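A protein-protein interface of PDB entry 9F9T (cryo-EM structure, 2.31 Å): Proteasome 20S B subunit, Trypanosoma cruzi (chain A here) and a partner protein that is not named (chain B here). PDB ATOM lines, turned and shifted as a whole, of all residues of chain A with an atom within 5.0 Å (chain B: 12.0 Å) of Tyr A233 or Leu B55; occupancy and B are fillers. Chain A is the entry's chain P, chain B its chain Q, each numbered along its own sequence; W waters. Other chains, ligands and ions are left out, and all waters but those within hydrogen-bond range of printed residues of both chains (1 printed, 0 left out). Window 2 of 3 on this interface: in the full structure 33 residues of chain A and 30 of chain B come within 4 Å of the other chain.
OD2 of Asp B57 is in salt-bridge range of NZ of Lys A94 (2.7 Å).
The backbone carbonyl oxygen (O) of Ala A212 is in hydrogen-bond range of the backbone NH (N) of Asp B57.
The side-chain amino group (NZ) of Lys A214 is in hydrogen-bond range of the backbone carbonyl oxygen (O) of Ser B54, 3.5 Å away.
N of Lys A214 is in hydrogen-bond range of O of Leu B55 (2.7 Å).
N of Lys A94 lies within hydrogen-bond range of O of Lys A214 (2.8 Å).
O of Lys A94 is in hydrogen-bond range of OH of Tyr A233, at 3.0 Å.
The side-chain amide oxygen of Asn B53 sits close to the backbone NH of Leu B55.
Among the printed residues, pairs that only touch across the chains: Lys A214 with Phe B56 (3.3 Å), Trp A213 with Phe B56 (3.4 Å), Trp A213 with Asn B53 (3.5 Å), Trp A213 with Leu B55 (3.6 Å), Trp A213 with Asp B57 (3.7 Å), Glu A230 with Asn B53 (3.7 Å), Ala A215 with Leu B55 (3.7 Å), Glu A230 with Leu B55 (3.9 Å), Lys A214 with Asp B57 (3.9 Å), Glu A230 with Ser B54 (3.9 Å) and Tyr A233 with Leu B55 (3.9 Å).
No residue of chain B comes within 4 Å of Val A93.
Lys A94 touches just one residue of chain B: Asp B57.
Ala A212 touches one residue of chain B.
Lys A214 touches just these residues of chain B: Ser B54, Leu B55, Phe B56 and Asp B57.
Ala A215 touches just one residue of chain B: Leu B55 (3.7 Å).
No residue of chain B comes within 4 Å of Leu A229.
Of chain B, only Asn B53 (3.7 Å), Ser B54 (3.9 Å) and Leu B55 (3.9 Å) come within 4 Å of Glu A230.
Of chain B, only Leu B55 comes within 4 Å of Tyr A233.
Thr A234 touches none of the printed residues of chain B.
No residue of chain B comes within 4 Å of Asn A235.
No residue of chain B comes within 4 Å of Met A237.
Gln B52 touches none of the printed residues of chain A.
Printed residues of chain A within 4 Å of Asn B53: Trp A213 and Glu A230.
Of the printed residues of chain A, Ser B54 touches Lys A214 and Glu A230.
Leu B55 touches just these residues of chain A: Trp A213, Lys A214, Ala A215, Glu A230 and Tyr A233.
Of the printed residues of chain A, Phe B56 touches Trp A213 and Lys A214.
Printed residues of chain A within 4 Å of Asp B57: Lys A94, Ala A212, Trp A213 and Lys A214.
Asn B60 touches none of the printed residues of chain A.
The nearest residue of chain B that does not touch Tyr A233 is Ser B54 (6.1 Å).
The nearest residue of chain A that does not touch Leu B55 is Lys A226 (4.2 Å).
The nearest printed residue of chain A that does not touch Phe B56 is Ala A212 (4.1 Å).
Of the 13 printed residues of chain B, 5 touch a printed residue of chain A.
Printed residues of chain B that touch a printed residue of chain A: Asn B53, Ser B54, Leu B55, Phe B56 and Asp B57.
Hydrophobic or aromatic side chains of chain B that line the printed part of chain A: Leu B55 and Phe B56.
Of the 15 printed residues of chain A, 7 touch a printed residue of chain B.
Hydrophobic or aromatic side chains of chain A within 4 Å of the printed part of chain B: Ala A212, Trp A213 and Tyr A233.
Among the printed residues, 15 pairs touch across the chains.
Among the printed residues, Asp or Glu carboxylates within 4 Å of a Lys or Arg side-chain nitrogen of the other chain: Lys A94 with Asp B57 (2.7 Å).
Water W1 lies within hydrogen-bond range of O of Trp A213 and OD2 of Asp B57.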
ATOM      1  N   VAL A  93      26.798   0.434 -35.209  1.00  0.00           N
ATOM      2  CA  VAL A  93      26.727  -1.008 -35.206  1.00  0.00           C
ATOM      3  C   VAL A  93      28.096  -1.645 -35.270  1.00  0.00           C
ATOM      4  O   VAL A  93      28.832  -1.445 -36.210  1.00  0.00           O
ATOM      5  CB  VAL A  93      25.844  -1.515 -36.355  1.00  0.00           C
ATOM      6  CG1 VAL A  93      25.887  -3.012 -36.448  1.00  0.00           C
ATOM      7  CG2 VAL A  93      24.417  -1.079 -36.163  1.00  0.00           C
ATOM      8  N   LYS A  94      28.362  -2.542 -34.325  1.00  0.00           N
ATOM      9  CA  LYS A  94      29.635  -3.243 -34.253  1.00  0.00           C
ATOM     10  C   LYS A  94      29.465  -4.658 -34.776  1.00  0.00           C
ATOM     11  O   LYS A  94      28.733  -5.441 -34.191  1.00  0.00           O
ATOM     12  CB  LYS A  94      30.148  -3.267 -32.825  1.00  0.00           C
ATOM     13  CG  LYS A  94      31.477  -3.969 -32.680  1.00  0.00           C
ATOM     14  CD  LYS A  94      31.971  -4.060 -31.266  1.00  0.00           C
ATOM     15  CE  LYS A  94      32.442  -5.467 -30.963  1.00  0.00           C
ATOM     16  NZ  LYS A  94      33.480  -5.479 -29.910  1.00  0.00           N
ATOM     17  N   ALA A 212      30.264   0.984 -23.497  1.00  0.00           N
ATOM     18  CA  ALA A 212      30.555   0.276 -24.712  1.00  0.00           C
ATOM     19  C   ALA A 212      29.287  -0.391 -25.213  1.00  0.00           C
ATOM     20  O   ALA A 212      28.519  -0.892 -24.411  1.00  0.00           O
ATOM     21  CB  ALA A 212      31.649  -0.737 -24.455  1.00  0.00           C
ATOM     22  N   TRP A 213      29.066  -0.401 -26.528  1.00  0.00           N
ATOM     23  CA  TRP A 213      27.856  -1.011 -27.053  1.00  0.00           C
ATOM     24  C   TRP A 213      28.180  -1.921 -28.212  1.00  0.00           C
ATOM     25  O   TRP A 213      29.240  -1.809 -28.797  1.00  0.00           O
ATOM     26  CB  TRP A 213      26.875   0.046 -27.538  1.00  0.00           C
ATOM     27  CG  TRP A 213      26.215   0.863 -26.470  1.00  0.00           C
ATOM     28  CD1 TRP A 213      26.543   2.109 -26.064  1.00  0.00           C
ATOM     29  CD2 TRP A 213      24.988   0.561 -25.811  1.00  0.00           C
ATOM     30  NE1 TRP A 213      25.675   2.574 -25.123  1.00  0.00           N
ATOM     31  CE2 TRP A 213      24.689   1.661 -24.969  1.00  0.00           C
ATOM     32  CE3 TRP A 213      24.096  -0.511 -25.875  1.00  0.00           C
ATOM     33  CZ2 TRP A 213      23.563   1.700 -24.160  1.00  0.00           C
ATOM     34  CZ3 TRP A 213      22.943  -0.435 -25.123  1.00  0.00           C
ATOM     35  CH2 TRP A 213      22.691   0.643 -24.276  1.00  0.00           C
ATOM     36  N   LYS A 214      27.280  -2.863 -28.497  1.00  0.00           N
ATOM     37  CA  LYS A 214      27.345  -3.667 -29.715  1.00  0.00           C
ATOM     38  C   LYS A 214      26.578  -2.909 -30.781  1.00  0.00           C
ATOM     39  O   LYS A 214      26.921  -2.994 -31.960  1.00  0.00           O
ATOM     40  CB  LYS A 214      26.730  -5.064 -29.559  1.00  0.00           C
ATOM     41  CG  LYS A 214      27.578  -6.035 -28.737  1.00  0.00           C
ATOM     42  CD  LYS A 214      26.834  -7.286 -28.379  1.00  0.00           C
ATOM     43  CE  LYS A 214      27.626  -8.257 -27.538  1.00  0.00           C
ATOM     44  NZ  LYS A 214      26.691  -9.126 -26.773  1.00  0.00           N
ATOM     45  N   ALA A 215      25.509  -2.224 -30.346  1.00  0.00           N
ATOM     46  CA  ALA A 215      24.768  -1.416 -31.296  1.00  0.00           C
ATOM     47  C   ALA A 215      23.879  -0.415 -30.564  1.00  0.00           C
ATOM     48  O   ALA A 215      23.296  -0.770 -29.559  1.00  0.00           O
ATOM     49  CB  ALA A 215      23.980  -2.326 -32.155  1.00  0.00           C
ATOM     50  N   LYS A 226      16.584   1.640 -31.497  1.00  0.00           N
ATOM     51  CA  LYS A 226      17.238   0.660 -30.614  1.00  0.00           C
ATOM     52  C   LYS A 226      16.423  -0.635 -30.522  1.00  0.00           C
ATOM     53  O   LYS A 226      16.994  -1.725 -30.531  1.00  0.00           O
ATOM     54  CB  LYS A 226      17.491   1.198 -29.193  1.00  0.00           C
ATOM     55  CG  LYS A 226      18.925   1.656 -28.881  1.00  0.00           C
ATOM     56  CD  LYS A 226      19.099   2.407 -27.540  1.00  0.00           C
ATOM     57  CE  LYS A 226      18.107   3.534 -27.365  1.00  0.00           C
ATOM     58  NZ  LYS A 226      18.345   4.338 -26.141  1.00  0.00           N
ATOM     59  N   LEU A 229      17.103  -2.535 -33.609  1.00  0.00           N
ATOM     60  CA  LEU A 229      18.422  -3.137 -33.669  1.00  0.00           C
ATOM     61  C   LEU A 229      18.510  -4.334 -32.731  1.00  0.00           C
ATOM     62  O   LEU A 229      19.318  -5.218 -32.989  1.00  0.00           O
ATOM     63  CB  LEU A 229      19.486  -2.118 -33.267  1.00  0.00           C
ATOM     64  CG  LEU A 229      19.692  -0.964 -34.228  1.00  0.00           C
ATOM     65  CD1 LEU A 229      20.529   0.120 -33.562  1.00  0.00           C
ATOM     66  CD2 LEU A 229      20.332  -1.461 -35.516  1.00  0.00           C
ATOM     67  N   GLU A 230      17.755  -4.331 -31.622  1.00  0.00           N
ATOM     68  CA  GLU A 230      17.651  -5.494 -30.739  1.00  0.00           C
ATOM     69  C   GLU A 230      17.368  -6.736 -31.581  1.00  0.00           C
ATOM     70  O   GLU A 230      18.086  -7.729 -31.478  1.00  0.00           O
ATOM     71  CB  GLU A 230      16.481  -5.338 -29.757  1.00  0.00           C
ATOM     72  CG  GLU A 230      16.831  -5.499 -28.290  1.00  0.00           C
ATOM     73  CD  GLU A 230      16.619  -4.234 -27.460  1.00  0.00           C
ATOM     74  OE1 GLU A 230      16.638  -4.328 -26.207  1.00  0.00           O
ATOM     75  OE2 GLU A 230      16.476  -3.149 -28.055  1.00  0.00           O
ATOM     76  N   LYS A 231      16.353  -6.618 -32.457  1.00  0.00           N
ATOM     77  CA  LYS A 231      15.832  -7.717 -33.261  1.00  0.00           C
ATOM     78  C   LYS A 231      16.802  -8.165 -34.358  1.00  0.00           C
ATOM     79  O   LYS A 231      17.009  -9.358 -34.548  1.00  0.00           O
ATOM     80  CB  LYS A 231      14.482  -7.332 -33.871  1.00  0.00           C
ATOM     81  CG  LYS A 231      13.297  -7.518 -32.933  1.00  0.00           C
ATOM     82  CD  LYS A 231      11.953  -7.599 -33.649  1.00  0.00           C
ATOM     83  CE  LYS A 231      11.413  -6.246 -34.054  1.00  0.00           C
ATOM     84  NZ  LYS A 231      11.001  -5.456 -32.867  1.00  0.00           N
ATOM     85  N   ARG A 232      17.417  -7.229 -35.071  1.00  0.00           N
ATOM     86  CA  ARG A 232      18.157  -7.579 -36.272  1.00  0.00           C
ATOM     87  C   ARG A 232      19.653  -7.799 -36.003  1.00  0.00           C
ATOM     88  O   ARG A 232      20.372  -8.188 -36.923  1.00  0.00           O
ATOM     89  CB  ARG A 232      17.935  -6.507 -37.351  1.00  0.00           C
ATOM     90  CG  ARG A 232      16.479  -6.076 -37.512  1.00  0.00           C
ATOM     91  CD  ARG A 232      16.050  -5.757 -38.938  1.00  0.00           C
ATOM     92  NE  ARG A 232      17.191  -5.583 -39.834  1.00  0.00           N
ATOM     93  CZ  ARG A 232      17.300  -6.126 -41.047  1.00  0.00           C
ATOM     94  NH1 ARG A 232      18.497  -6.289 -41.591  1.00  0.00           N
ATOM     95  NH2 ARG A 232      16.225  -6.578 -41.672  1.00  0.00           N
ATOM     96  N   TYR A 233      20.132  -7.585 -34.767  1.00  0.00           N
ATOM     97  CA  TYR A 233      21.569  -7.618 -34.506  1.00  0.00           C
ATOM     98  C   TYR A 233      21.977  -9.048 -34.134  1.00  0.00           C
ATOM     99  O   TYR A 233      21.369  -9.664 -33.260  1.00  0.00           O
ATOM    100  CB  TYR A 233      22.005  -6.624 -33.404  1.00  0.00           C
ATOM    101  CG  TYR A 233      23.470  -6.793 -33.024  1.00  0.00           C
ATOM    102  CD1 TYR A 233      24.446  -6.146 -33.725  1.00  0.00           C
ATOM    103  CD2 TYR A 233      23.888  -7.730 -32.086  1.00  0.00           C
ATOM    104  CE1 TYR A 233      25.786  -6.344 -33.450  1.00  0.00           C
ATOM    105  CE2 TYR A 233      25.230  -7.955 -31.808  1.00  0.00           C
ATOM    106  CZ  TYR A 233      26.195  -7.253 -32.497  1.00  0.00           C
ATOM    107  OH  TYR A 233      27.549  -7.400 -32.265  1.00  0.00           O
ATOM    108  N   THR A 234      23.061  -9.546 -34.755  1.00  0.00           N
ATOM    109  CA  THR A 234      23.635 -10.846 -34.402  1.00  0.00           C
ATOM    110  C   THR A 234      25.143 -10.715 -34.169  1.00  0.00           C
ATOM    111  O   THR A 234      25.792  -9.822 -34.724  1.00  0.00           O
ATOM    112  CB  THR A 234      23.316 -11.909 -35.471  1.00  0.00           C
ATOM    113  OG1 THR A 234      23.921 -11.558 -36.716  1.00  0.00           O
ATOM    114  CG2 THR A 234      21.831 -12.105 -35.701  1.00  0.00           C
ATOM    115  N   ASN A 235      25.712 -11.632 -33.369  1.00  0.00           N
ATOM    116  CA  ASN A 235      27.124 -11.561 -33.001  1.00  0.00           C
ATOM    117  C   ASN A 235      28.036 -11.959 -34.164  1.00  0.00           C
ATOM    118  O   ASN A 235      29.262 -11.892 -34.032  1.00  0.00           O
ATOM    119  CB  ASN A 235      27.435 -12.389 -31.748  1.00  0.00           C
ATOM    120  CG  ASN A 235      27.067 -11.681 -30.455  1.00  0.00           C
ATOM    121  OD1 ASN A 235      27.878 -10.946 -29.894  1.00  0.00           O
ATOM    122  ND2 ASN A 235      25.858 -11.909 -29.967  1.00  0.00           N
ATOM    123  N   MET A 237      27.531 -10.872 -37.545  1.00  0.00           N
ATOM    124  CA  MET A 237      27.343  -9.998 -38.688  1.00  0.00           C
ATOM    125  C   MET A 237      28.702  -9.714 -39.316  1.00  0.00           C
ATOM    126  O   MET A 237      29.660  -9.434 -38.602  1.00  0.00           O
ATOM    127  CB  MET A 237      26.767  -8.642 -38.283  1.00  0.00           C
ATOM    128  CG  MET A 237      25.313  -8.649 -37.960  1.00  0.00           C
ATOM    129  SD  MET A 237      24.764  -6.933 -37.828  1.00  0.00           S
ATOM    130  CE  MET A 237      23.177  -7.067 -38.652  1.00  0.00           C
ATOM    131  N   GLY B  50      23.292  -2.198 -12.911  1.00  0.00           N
ATOM    132  CA  GLY B  50      22.107  -1.898 -13.707  1.00  0.00           C
ATOM    133  C   GLY B  50      21.592  -3.137 -14.449  1.00  0.00           C
ATOM    134  O   GLY B  50      22.178  -4.217 -14.348  1.00  0.00           O
ATOM    135  N   VAL B  51      20.499  -2.982 -15.208  1.00  0.00           N
ATOM    136  CA  VAL B  51      19.872  -4.133 -15.848  1.00  0.00           C
ATOM    137  C   VAL B  51      20.516  -4.365 -17.218  1.00  0.00           C
ATOM    138  O   VAL B  51      20.746  -3.419 -17.974  1.00  0.00           O
ATOM    139  CB  VAL B  51      18.339  -3.992 -15.939  1.00  0.00           C
ATOM    140  CG1 VAL B  51      17.680  -5.314 -16.321  1.00  0.00           C
ATOM    141  CG2 VAL B  51      17.741  -3.447 -14.649  1.00  0.00           C
ATOM    142  N   GLN B  52      20.760  -5.650 -17.526  1.00  0.00           N
ATOM    143  CA  GLN B  52      21.674  -6.060 -18.582  1.00  0.00           C
ATOM    144  C   GLN B  52      20.951  -6.151 -19.928  1.00  0.00           C
ATOM    145  O   GLN B  52      20.201  -7.093 -20.182  1.00  0.00           O
ATOM    146  CB  GLN B  52      22.341  -7.382 -18.203  1.00  0.00           C
ATOM    147  CG  GLN B  52      23.157  -7.287 -16.916  1.00  0.00           C
ATOM    148  CD  GLN B  52      24.416  -6.460 -17.050  1.00  0.00           C
ATOM    149  OE1 GLN B  52      24.459  -5.283 -16.699  1.00  0.00           O
ATOM    150  NE2 GLN B  52      25.461  -7.078 -17.575  1.00  0.00           N
ATOM    151  N   ASN B  53      21.210  -5.144 -20.771  1.00  0.00           N
ATOM    152  CA  ASN B  53      20.742  -5.050 -22.142  1.00  0.00           C
ATOM    153  C   ASN B  53      21.535  -6.037 -23.009  1.00  0.00           C
ATOM    154  O   ASN B  53      22.755  -6.146 -22.899  1.00  0.00           O
ATOM    155  CB  ASN B  53      20.890  -3.583 -22.564  1.00  0.00           C
ATOM    156  CG  ASN B  53      20.270  -3.241 -23.900  1.00  0.00           C
ATOM    157  OD1 ASN B  53      20.077  -4.094 -24.761  1.00  0.00           O
ATOM    158  ND2 ASN B  53      19.991  -1.963 -24.099  1.00  0.00           N
ATOM    159  N   SER B  54      20.849  -6.772 -23.891  1.00  0.00           N
ATOM    160  CA  SER B  54      21.521  -7.684 -24.815  1.00  0.00           C
ATOM    161  C   SER B  54      22.656  -6.986 -25.566  1.00  0.00           C
ATOM    162  O   SER B  54      23.670  -7.619 -25.890  1.00  0.00           O
ATOM    163  CB  SER B  54      20.537  -8.245 -25.832  1.00  0.00           C
ATOM    164  OG  SER B  54      19.960  -7.202 -26.629  1.00  0.00           O
ATOM    165  N   LEU B  55      22.443  -5.692 -25.858  1.00  0.00           N
ATOM    166  CA  LEU B  55      23.289  -4.931 -26.759  1.00  0.00           C
ATOM    167  C   LEU B  55      24.551  -4.326 -26.094  1.00  0.00           C
ATOM    168  O   LEU B  55      25.426  -3.837 -26.798  1.00  0.00           O
ATOM    169  CB  LEU B  55      22.406  -3.880 -27.441  1.00  0.00           C
ATOM    170  CG  LEU B  55      21.501  -4.425 -28.552  1.00  0.00           C
ATOM    171  CD1 LEU B  55      20.601  -3.347 -29.172  1.00  0.00           C
ATOM    172  CD2 LEU B  55      22.313  -5.071 -29.649  1.00  0.00           C
ATOM    173  N   PHE B  56      24.725  -4.421 -24.774  1.00  0.00           N
ATOM    174  CA  PHE B  56      25.989  -4.052 -24.163  1.00  0.00           C
ATOM    175  C   PHE B  56      27.162  -4.839 -24.747  1.00  0.00           C
ATOM    176  O   PHE B  56      27.001  -5.837 -25.432  1.00  0.00           O
ATOM    177  CB  PHE B  56      25.980  -4.259 -22.650  1.00  0.00           C
ATOM    178  CG  PHE B  56      25.161  -3.268 -21.877  1.00  0.00           C
ATOM    179  CD1 PHE B  56      24.790  -2.044 -22.432  1.00  0.00           C
ATOM    180  CD2 PHE B  56      24.754  -3.561 -20.582  1.00  0.00           C
ATOM    181  CE1 PHE B  56      24.041  -1.127 -21.708  1.00  0.00           C
ATOM    182  CE2 PHE B  56      23.979  -2.650 -19.872  1.00  0.00           C
ATOM    183  CZ  PHE B  56      23.630  -1.436 -20.433  1.00  0.00           C
ATOM    184  N   ASP B  57      28.362  -4.333 -24.482  1.00  0.00           N
ATOM    185  CA  ASP B  57      29.567  -4.979 -24.949  1.00  0.00           C
ATOM    186  C   ASP B  57      30.596  -4.760 -23.877  1.00  0.00           C
ATOM    187  O   ASP B  57      30.355  -3.942 -22.994  1.00  0.00           O
ATOM    188  CB  ASP B  57      30.112  -4.412 -26.264  1.00  0.00           C
ATOM    189  CG  ASP B  57      31.131  -5.295 -26.985  1.00  0.00           C
ATOM    190  OD1 ASP B  57      31.207  -6.520 -26.667  1.00  0.00           O
ATOM    191  OD2 ASP B  57      31.847  -4.755 -27.873  1.00  0.00           O
ATOM    192  N   SER B  58      31.672  -5.538 -23.977  1.00  0.00           N
ATOM    193  CA  SER B  58      32.848  -5.397 -23.151  1.00  0.00           C
ATOM    194  C   SER B  58      33.765  -4.392 -23.818  1.00  0.00           C
ATOM    195  O   SER B  58      33.743  -4.312 -25.034  1.00  0.00           O
ATOM    196  CB  SER B  58      33.574  -6.749 -22.990  1.00  0.00           C
ATOM    197  OG  SER B  58      34.556  -6.711 -21.953  1.00  0.00           O
ATOM    198  N   GLU B  59      34.601  -3.715 -23.014  1.00  0.00           N
ATOM    199  CA  GLU B  59      35.772  -2.982 -23.482  1.00  0.00           C
ATOM    200  C   GLU B  59      36.863  -3.935 -23.995  1.00  0.00           C
ATOM    201  O   GLU B  59      37.741  -3.534 -24.748  1.00  0.00           O
ATOM    202  CB  GLU B  59      36.327  -2.082 -22.362  1.00  0.00           C
ATOM    203  CG  GLU B  59      35.369  -0.945 -21.943  1.00  0.00           C
ATOM    204  CD  GLU B  59      35.979   0.215 -21.150  1.00  0.00           C
ATOM    205  OE1 GLU B  59      35.863   0.204 -19.894  1.00  0.00           O
ATOM    206  OE2 GLU B  59      36.513   1.158 -21.770  1.00  0.00           O
ATOM    207  N   ASN B  60      36.842  -5.179 -23.545  1.00  0.00           N
ATOM    208  CA  ASN B  60      37.857  -6.161 -23.904  1.00  0.00           C
ATOM    209  C   ASN B  60      39.265  -5.686 -23.514  1.00  0.00           C
ATOM    210  O   ASN B  60      40.179  -5.680 -24.334  1.00  0.00           O
ATOM    211  CB  ASN B  60      37.706  -6.585 -25.369  1.00  0.00           C
ATOM    212  CG  ASN B  60      38.497  -7.845 -25.673  1.00  0.00           C
ATOM    213  OD1 ASN B  60      38.453  -8.803 -24.899  1.00  0.00           O
ATOM    214  ND2 ASN B  60      39.272  -7.835 -26.751  1.00  0.00           N
ATOM    215  N   GLU B  69      32.632  -2.647 -13.506  1.00  0.00           N
ATOM    216  CA  GLU B  69      31.662  -1.575 -13.571  1.00  0.00           C
ATOM    217  C   GLU B  69      31.739  -0.733 -12.297  1.00  0.00           C
ATOM    218  O   GLU B  69      31.418   0.457 -12.330  1.00  0.00           O
ATOM    219  CB  GLU B  69      30.274  -2.162 -13.860  1.00  0.00           C
ATOM    220  CG  GLU B  69      29.895  -2.207 -15.352  1.00  0.00           C
ATOM    221  CD  GLU B  69      30.876  -2.809 -16.364  1.00  0.00           C
ATOM    222  OE1 GLU B  69      31.902  -3.392 -15.949  1.00  0.00           O
ATOM    223  OE2 GLU B  69      30.613  -2.679 -17.586  1.00  0.00           O
ATOM    224  N   GLU B 214      24.876 -12.270 -13.426  1.00  0.00           N
ATOM    225  CA  GLU B 214      25.140 -11.194 -14.370  1.00  0.00           C
ATOM    226  C   GLU B 214      24.719  -9.842 -13.793  1.00  0.00           C
ATOM    227  O   GLU B 214      24.852  -8.834 -14.477  1.00  0.00           O
ATOM    228  CB  GLU B 214      24.364 -11.400 -15.675  1.00  0.00           C
ATOM    229  CG  GLU B 214      24.571 -12.749 -16.350  1.00  0.00           C
ATOM    230  CD  GLU B 214      23.852 -12.905 -17.685  1.00  0.00           C
ATOM    231  OE1 GLU B 214      23.367 -11.886 -18.227  1.00  0.00           O
ATOM    232  OE2 GLU B 214      23.761 -14.049 -18.177  1.00  0.00           O
HETATM  233  O   HOH W   1      31.730  -1.615 -28.218  1.00  0.00           O
